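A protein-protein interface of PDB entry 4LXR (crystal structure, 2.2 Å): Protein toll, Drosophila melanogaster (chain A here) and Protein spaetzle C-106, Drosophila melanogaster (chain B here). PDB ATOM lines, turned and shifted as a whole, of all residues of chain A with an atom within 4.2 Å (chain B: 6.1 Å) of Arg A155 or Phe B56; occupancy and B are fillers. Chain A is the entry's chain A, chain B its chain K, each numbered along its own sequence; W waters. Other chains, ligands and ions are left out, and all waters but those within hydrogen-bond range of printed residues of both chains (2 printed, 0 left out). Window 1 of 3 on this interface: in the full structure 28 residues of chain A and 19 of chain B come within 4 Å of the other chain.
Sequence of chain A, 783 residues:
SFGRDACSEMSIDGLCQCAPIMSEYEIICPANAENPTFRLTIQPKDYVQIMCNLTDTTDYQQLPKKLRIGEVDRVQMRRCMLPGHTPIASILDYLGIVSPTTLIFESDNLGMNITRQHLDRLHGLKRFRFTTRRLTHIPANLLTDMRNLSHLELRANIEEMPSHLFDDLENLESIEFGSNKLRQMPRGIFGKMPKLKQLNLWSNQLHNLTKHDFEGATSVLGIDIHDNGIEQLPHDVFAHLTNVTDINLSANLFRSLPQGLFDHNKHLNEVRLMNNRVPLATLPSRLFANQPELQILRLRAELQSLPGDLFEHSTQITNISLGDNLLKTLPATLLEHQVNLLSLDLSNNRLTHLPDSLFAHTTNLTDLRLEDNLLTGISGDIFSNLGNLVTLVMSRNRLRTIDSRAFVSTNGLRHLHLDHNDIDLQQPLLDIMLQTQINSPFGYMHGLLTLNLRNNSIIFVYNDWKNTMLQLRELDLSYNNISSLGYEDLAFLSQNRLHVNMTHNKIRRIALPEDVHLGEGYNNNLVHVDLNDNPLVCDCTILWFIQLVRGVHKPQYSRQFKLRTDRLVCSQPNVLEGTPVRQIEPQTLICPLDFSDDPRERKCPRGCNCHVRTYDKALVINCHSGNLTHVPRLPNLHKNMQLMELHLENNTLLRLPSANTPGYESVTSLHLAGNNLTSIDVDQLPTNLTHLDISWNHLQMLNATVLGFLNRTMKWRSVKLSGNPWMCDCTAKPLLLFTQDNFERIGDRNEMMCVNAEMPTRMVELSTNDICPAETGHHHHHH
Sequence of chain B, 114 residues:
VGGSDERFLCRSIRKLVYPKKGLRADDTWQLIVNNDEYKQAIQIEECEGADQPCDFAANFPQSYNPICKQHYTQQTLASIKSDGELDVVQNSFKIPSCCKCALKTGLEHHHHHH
The guanidinium group (NH1) of Arg A155 is in salt-bridge range of the side-chain carboxylate (OD1) of Asp B55, 2.9 Å away.
Arg A155 touches Phe B56. Trp A202 touches Phe B56.
N of Arg A155 is in hydrogen-bond range of O of Phe A130, at 2.9 Å. N of Thr A132 lies within hydrogen-bond range of O of Arg A155. N of Ser A179 is in hydrogen-bond range of O of Trp A202 (2.8 Å). The backbone carbonyl oxygen (O) of Leu B9 lies within hydrogen-bond range of the backbone NH (N) of Asp B55 (2.8 Å).
Printed residues of chain A that touch a printed residue of chain B: Arg A155 and Trp A202. Hydrophobic or aromatic side chains of chain A that line the printed part of chain B: Trp A202. Among the printed residues, Asp or Glu carboxylates within 4 Å of a Lys or Arg side-chain nitrogen of the other chain: Arg A155 with Asp B55.
Arg A155 touches just these residues of chain B: Asp B55 and Phe B56. Printed residues of chain B within 4 Å of Trp A202: Phe B56 (3.8 Å). Of the printed residues of chain A, Asp B55 touches Arg A155 (2.9 Å). Printed residues of chain A within 4 Å of Phe B56: Arg A155 (3.8 Å) and Trp A202 (3.8 Å). The nearest residue of chain B that does not touch Arg A155 is Arg B7 (5.0 Å). The nearest printed residue of chain A that does not touch Phe B56 is Ser A179 (7.2 Å). The nearest printed residue of chain B that does not touch Trp A202 is Asp B55 (4.1 Å).
Water W2 lies within hydrogen-bond range of the side-chain carboxylate (OD2) of Asp B55 (2.8 Å), the guanidinium group (NH1) of Arg A155 (3.3 Å) and the guanidinium group (NH1) of Arg B7 (3.3 Å). Water W1 lies within hydrogen-bond range of OG1 of Thr A131, NE of Arg A155 and NH1 of Arg B7.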
ATOM      1  N   PHE A 130      -0.821  12.543 -33.146  1.00  0.00           N
ATOM      2  CA  PHE A 130      -2.152  13.127 -33.117  1.00  0.00           C
ATOM      3  C   PHE A 130      -2.263  13.993 -31.875  1.00  0.00           C
ATOM      4  O   PHE A 130      -2.020  13.529 -30.750  1.00  0.00           O
ATOM      5  CB  PHE A 130      -3.231  12.029 -33.079  1.00  0.00           C
ATOM      6  CG  PHE A 130      -4.634  12.560 -33.002  1.00  0.00           C
ATOM      7  CD1 PHE A 130      -5.100  13.472 -33.951  1.00  0.00           C
ATOM      8  CD2 PHE A 130      -5.489  12.142 -32.002  1.00  0.00           C
ATOM      9  CE1 PHE A 130      -6.397  13.977 -33.895  1.00  0.00           C
ATOM     10  CE2 PHE A 130      -6.807  12.637 -31.927  1.00  0.00           C
ATOM     11  CZ  PHE A 130      -7.263  13.554 -32.875  1.00  0.00           C
ATOM     12  N   THR A 131      -2.685  15.233 -32.060  1.00  0.00           N
ATOM     13  CA  THR A 131      -2.633  16.195 -30.965  1.00  0.00           C
ATOM     14  C   THR A 131      -3.852  17.083 -31.030  1.00  0.00           C
ATOM     15  O   THR A 131      -4.162  17.645 -32.089  1.00  0.00           O
ATOM     16  CB  THR A 131      -1.356  17.052 -31.080  1.00  0.00           C
ATOM     17  OG1 THR A 131      -0.208  16.228 -30.814  1.00  0.00           O
ATOM     18  CG2 THR A 131      -1.381  18.233 -30.109  1.00  0.00           C
ATOM     19  N   THR A 132      -4.552  17.215 -29.911  1.00  0.00           N
ATOM     20  CA  THR A 132      -5.747  18.052 -29.883  1.00  0.00           C
ATOM     21  C   THR A 132      -6.034  18.482 -28.457  1.00  0.00           C
ATOM     22  O   THR A 132      -5.667  17.785 -27.520  1.00  0.00           O
ATOM     23  CB  THR A 132      -6.995  17.319 -30.450  1.00  0.00           C
ATOM     24  OG1 THR A 132      -8.111  18.222 -30.471  1.00  0.00           O
ATOM     25  CG2 THR A 132      -7.369  16.092 -29.596  1.00  0.00           C
ATOM     26  N   LEU A 154       0.533  10.556 -28.922  1.00  0.00           N
ATOM     27  CA  LEU A 154      -0.892  10.831 -28.845  1.00  0.00           C
ATOM     28  C   LEU A 154      -1.062  11.783 -27.717  1.00  0.00           C
ATOM     29  O   LEU A 154      -0.579  11.553 -26.612  1.00  0.00           O
ATOM     30  CB  LEU A 154      -1.730   9.555 -28.571  1.00  0.00           C
ATOM     31  CG  LEU A 154      -1.695   8.485 -29.644  1.00  0.00           C
ATOM     32  CD1 LEU A 154      -2.458   7.228 -29.177  1.00  0.00           C
ATOM     33  CD2 LEU A 154      -2.312   9.030 -30.909  1.00  0.00           C
ATOM     34  N   ARG A 155      -1.771  12.861 -27.987  1.00  0.00           N
ATOM     35  CA  ARG A 155      -2.018  13.841 -26.963  1.00  0.00           C
ATOM     36  C   ARG A 155      -3.449  14.306 -27.089  1.00  0.00           C
ATOM     37  O   ARG A 155      -3.766  15.099 -27.974  1.00  0.00           O
ATOM     38  CB  ARG A 155      -1.080  15.043 -27.110  1.00  0.00           C
ATOM     39  CG  ARG A 155      -1.187  15.953 -25.912  1.00  0.00           C
ATOM     40  CD  ARG A 155      -0.258  17.095 -25.922  1.00  0.00           C
ATOM     41  NE  ARG A 155       1.167  16.795 -25.750  1.00  0.00           N
ATOM     42  CZ  ARG A 155       2.018  17.730 -25.331  1.00  0.00           C
ATOM     43  NH1 ARG A 155       1.530  18.921 -25.031  1.00  0.00           N
ATOM     44  NH2 ARG A 155       3.322  17.503 -25.196  1.00  0.00           N
ATOM     45  N   ALA A 156      -4.312  13.824 -26.200  1.00  0.00           N
ATOM     46  CA  ALA A 156      -5.728  14.128 -26.322  1.00  0.00           C
ATOM     47  C   ALA A 156      -6.495  14.009 -25.004  1.00  0.00           C
ATOM     48  O   ALA A 156      -7.639  13.528 -24.996  1.00  0.00           O
ATOM     49  CB  ALA A 156      -6.344  13.218 -27.371  1.00  0.00           C
ATOM     50  N   ASN A 157      -5.880  14.459 -23.906  1.00  0.00           N
ATOM     51  CA  ASN A 157      -6.447  14.300 -22.561  1.00  0.00           C
ATOM     52  C   ASN A 157      -6.928  12.873 -22.292  1.00  0.00           C
ATOM     53  O   ASN A 157      -7.997  12.662 -21.721  1.00  0.00           O
ATOM     54  CB  ASN A 157      -7.551  15.337 -22.276  1.00  0.00           C
ATOM     55  CG  ASN A 157      -6.962  16.740 -22.044  1.00  0.00           C
ATOM     56  OD1 ASN A 157      -6.518  17.049 -20.946  1.00  0.00           O
ATOM     57  ND2 ASN A 157      -6.893  17.556 -23.107  1.00  0.00           N
ATOM     58  N   GLY A 178       3.018  11.750 -23.106  1.00  0.00           N
ATOM     59  CA  GLY A 178       3.132  12.843 -22.166  1.00  0.00           C
ATOM     60  C   GLY A 178       1.949  13.793 -22.285  1.00  0.00           C
ATOM     61  O   GLY A 178       1.416  13.995 -23.372  1.00  0.00           O
ATOM     62  N   SER A 179       1.533  14.336 -21.150  1.00  0.00           N
ATOM     63  CA  SER A 179       0.501  15.365 -21.075  1.00  0.00           C
ATOM     64  C   SER A 179      -0.887  14.855 -21.434  1.00  0.00           C
ATOM     65  O   SER A 179      -1.613  15.445 -22.237  1.00  0.00           O
ATOM     66  CB  SER A 179       0.877  16.602 -21.903  1.00  0.00           C
ATOM     67  OG  SER A 179       0.225  17.742 -21.372  1.00  0.00           O
ATOM     68  N   ASN A 180      -1.259  13.747 -20.815  1.00  0.00           N
ATOM     69  CA  ASN A 180      -2.593  13.211 -20.972  1.00  0.00           C
ATOM     70  C   ASN A 180      -3.203  13.127 -19.601  1.00  0.00           C
ATOM     71  O   ASN A 180      -2.851  13.920 -18.719  1.00  0.00           O
ATOM     72  CB  ASN A 180      -2.562  11.858 -21.694  1.00  0.00           C
ATOM     73  CG  ASN A 180      -2.422  12.015 -23.203  1.00  0.00           C
ATOM     74  OD1 ASN A 180      -3.367  12.431 -23.887  1.00  0.00           O
ATOM     75  ND2 ASN A 180      -1.231  11.705 -23.731  1.00  0.00           N
ATOM     76  N   TRP A 202       5.189  11.431 -18.986  1.00  0.00           N
ATOM     77  CA  TRP A 202       5.238  12.618 -18.111  1.00  0.00           C
ATOM     78  C   TRP A 202       3.924  13.383 -18.161  1.00  0.00           C
ATOM     79  O   TRP A 202       3.165  13.273 -19.141  1.00  0.00           O
ATOM     80  CB  TRP A 202       6.424  13.538 -18.486  1.00  0.00           C
ATOM     81  CG  TRP A 202       6.480  13.848 -19.956  1.00  0.00           C
ATOM     82  CD1 TRP A 202       7.005  13.054 -20.939  1.00  0.00           C
ATOM     83  CD2 TRP A 202       5.974  15.012 -20.612  1.00  0.00           C
ATOM     84  NE1 TRP A 202       6.873  13.664 -22.172  1.00  0.00           N
ATOM     85  CE2 TRP A 202       6.237  14.868 -21.993  1.00  0.00           C
ATOM     86  CE3 TRP A 202       5.340  16.171 -20.168  1.00  0.00           C
ATOM     87  CZ2 TRP A 202       5.862  15.829 -22.928  1.00  0.00           C
ATOM     88  CZ3 TRP A 202       4.981  17.136 -21.101  1.00  0.00           C
ATOM     89  CH2 TRP A 202       5.247  16.961 -22.458  1.00  0.00           C
ATOM     90  N   ARG B   7      10.738  20.166 -32.193  1.00  0.00           N
ATOM     91  CA  ARG B   7       9.608  20.660 -31.440  1.00  0.00           C
ATOM     92  C   ARG B   7      10.020  21.978 -30.785  1.00  0.00           C
ATOM     93  O   ARG B   7      11.167  22.153 -30.402  1.00  0.00           O
ATOM     94  CB  ARG B   7       9.192  19.645 -30.379  1.00  0.00           C
ATOM     95  CG  ARG B   7       8.869  18.269 -30.929  1.00  0.00           C
ATOM     96  CD  ARG B   7       7.687  18.284 -31.916  1.00  0.00           C
ATOM     97  NE  ARG B   7       6.404  18.558 -31.272  1.00  0.00           N
ATOM     98  CZ  ARG B   7       5.678  17.634 -30.632  1.00  0.00           C
ATOM     99  NH1 ARG B   7       4.519  17.958 -30.080  1.00  0.00           N
ATOM    100  NH2 ARG B   7       6.127  16.387 -30.525  1.00  0.00           N
ATOM    101  N   PHE B   8       9.073  22.890 -30.651  1.00  0.00           N
ATOM    102  CA  PHE B   8       9.325  24.140 -29.983  1.00  0.00           C
ATOM    103  C   PHE B   8       8.384  24.309 -28.803  1.00  0.00           C
ATOM    104  O   PHE B   8       7.284  23.759 -28.791  1.00  0.00           O
ATOM    105  CB  PHE B   8       9.155  25.279 -30.979  1.00  0.00           C
ATOM    106  CG  PHE B   8      10.169  25.254 -32.071  1.00  0.00           C
ATOM    107  CD1 PHE B   8      11.460  25.709 -31.836  1.00  0.00           C
ATOM    108  CD2 PHE B   8       9.852  24.745 -33.321  1.00  0.00           C
ATOM    109  CE1 PHE B   8      12.409  25.685 -32.837  1.00  0.00           C
ATOM    110  CE2 PHE B   8      10.800  24.711 -34.324  1.00  0.00           C
ATOM    111  CZ  PHE B   8      12.077  25.179 -34.085  1.00  0.00           C
ATOM    112  N   LEU B   9       8.821  25.081 -27.818  1.00  0.00           N
ATOM    113  CA  LEU B   9       8.041  25.294 -26.596  1.00  0.00           C
ATOM    114  C   LEU B   9       6.767  26.080 -26.835  1.00  0.00           C
ATOM    115  O   LEU B   9       5.803  25.977 -26.065  1.00  0.00           O
ATOM    116  CB  LEU B   9       8.886  25.975 -25.522  1.00  0.00           C
ATOM    117  CG  LEU B   9       9.754  24.963 -24.772  1.00  0.00           C
ATOM    118  CD1 LEU B   9      10.862  24.416 -25.646  1.00  0.00           C
ATOM    119  CD2 LEU B   9      10.315  25.571 -23.506  1.00  0.00           C
ATOM    120  N   CYS B  54       3.947  27.390 -21.808  1.00  0.00           N
ATOM    121  CA  CYS B  54       4.802  26.713 -22.776  1.00  0.00           C
ATOM    122  C   CYS B  54       4.598  25.195 -22.713  1.00  0.00           C
ATOM    123  O   CYS B  54       4.202  24.652 -21.679  1.00  0.00           O
ATOM    124  CB  CYS B  54       6.283  27.071 -22.528  1.00  0.00           C
ATOM    125  SG  CYS B  54       6.652  28.854 -22.284  1.00  0.00           S
ATOM    126  N   ASP B  55       4.880  24.510 -23.816  1.00  0.00           N
ATOM    127  CA  ASP B  55       4.805  23.052 -23.856  1.00  0.00           C
ATOM    128  C   ASP B  55       6.153  22.537 -23.345  1.00  0.00           C
ATOM    129  O   ASP B  55       7.090  23.315 -23.224  1.00  0.00           O
ATOM    130  CB  ASP B  55       4.543  22.585 -25.293  1.00  0.00           C
ATOM    131  CG  ASP B  55       3.983  21.156 -25.372  1.00  0.00           C
ATOM    132  OD1 ASP B  55       3.980  20.416 -24.352  1.00  0.00           O
ATOM    133  OD2 ASP B  55       3.559  20.770 -26.486  1.00  0.00           O
ATOM    134  N   PHE B  56       6.245  21.246 -23.026  1.00  0.00           N
ATOM    135  CA  PHE B  56       7.508  20.638 -22.578  1.00  0.00           C
ATOM    136  C   PHE B  56       8.132  21.377 -21.404  1.00  0.00           C
ATOM    137  O   PHE B  56       9.347  21.381 -21.228  1.00  0.00           O
ATOM    138  CB  PHE B  56       8.502  20.540 -23.743  1.00  0.00           C
ATOM    139  CG  PHE B  56       7.894  19.940 -24.980  1.00  0.00           C
ATOM    140  CD1 PHE B  56       7.528  18.597 -25.004  1.00  0.00           C
ATOM    141  CD2 PHE B  56       7.651  20.721 -26.099  1.00  0.00           C
ATOM    142  CE1 PHE B  56       6.942  18.045 -26.118  1.00  0.00           C
ATOM    143  CE2 PHE B  56       7.067  20.176 -27.217  1.00  0.00           C
ATOM    144  CZ  PHE B  56       6.712  18.831 -27.233  1.00  0.00           C
ATOM    145  N   ALA B  57       7.292  21.986 -20.585  1.00  0.00           N
ATOM    146  CA  ALA B  57       7.796  22.857 -19.524  1.00  0.00           C
ATOM    147  C   ALA B  57       7.298  22.426 -18.148  1.00  0.00           C
ATOM    148  O   ALA B  57       7.095  23.263 -17.279  1.00  0.00           O
ATOM    149  CB  ALA B  57       7.410  24.308 -19.806  1.00  0.00           C
ATOM    150  N   ALA B  58       7.121  21.117 -17.960  1.00  0.00           N
ATOM    151  CA  ALA B  58       6.614  20.563 -16.706  1.00  0.00           C
ATOM    152  C   ALA B  58       7.710  20.226 -15.673  1.00  0.00           C
ATOM    153  O   ALA B  58       7.403  19.742 -14.585  1.00  0.00           O
ATOM    154  CB  ALA B  58       5.765  19.336 -16.989  1.00  0.00           C
ATOM    155  N   ASN B  59       8.972  20.453 -16.030  1.00  0.00           N
ATOM    156  CA  ASN B  59      10.113  20.247 -15.128  1.00  0.00           C
ATOM    157  C   ASN B  59      10.976  21.515 -14.963  1.00  0.00           C
ATOM    158  O   ASN B  59      12.187  21.490 -15.157  1.00  0.00           O
ATOM    159  CB  ASN B  59      10.993  19.061 -15.590  1.00  0.00           C
ATOM    160  CG  ASN B  59      12.115  18.734 -14.598  1.00  0.00           C
ATOM    161  OD1 ASN B  59      12.017  19.083 -13.420  1.00  0.00           O
ATOM    162  ND2 ASN B  59      13.183  18.050 -15.069  1.00  0.00           N
ATOM    163  N   PHE B  60      10.335  22.621 -14.607  1.00  0.00           N
ATOM    164  CA  PHE B  60      11.033  23.830 -14.191  1.00  0.00           C
ATOM    165  C   PHE B  60      10.546  24.119 -12.774  1.00  0.00           C
ATOM    166  O   PHE B  60       9.475  23.639 -12.396  1.00  0.00           O
ATOM    167  CB  PHE B  60      10.746  25.015 -15.145  1.00  0.00           C
ATOM    168  CG  PHE B  60      11.451  24.905 -16.493  1.00  0.00           C
ATOM    169  CD1 PHE B  60      12.802  25.219 -16.616  1.00  0.00           C
ATOM    170  CD2 PHE B  60      10.762  24.493 -17.620  1.00  0.00           C
ATOM    171  CE1 PHE B  60      13.450  25.120 -17.843  1.00  0.00           C
ATOM    172  CE2 PHE B  60      11.408  24.373 -18.863  1.00  0.00           C
ATOM    173  CZ  PHE B  60      12.749  24.693 -18.973  1.00  0.00           C
HETATM  174  O   HOH W   1       1.781  16.369 -28.628  1.00  0.00           O
HETATM  175  O   HOH W   2       2.042  19.132 -28.237  1.00  0.00           O
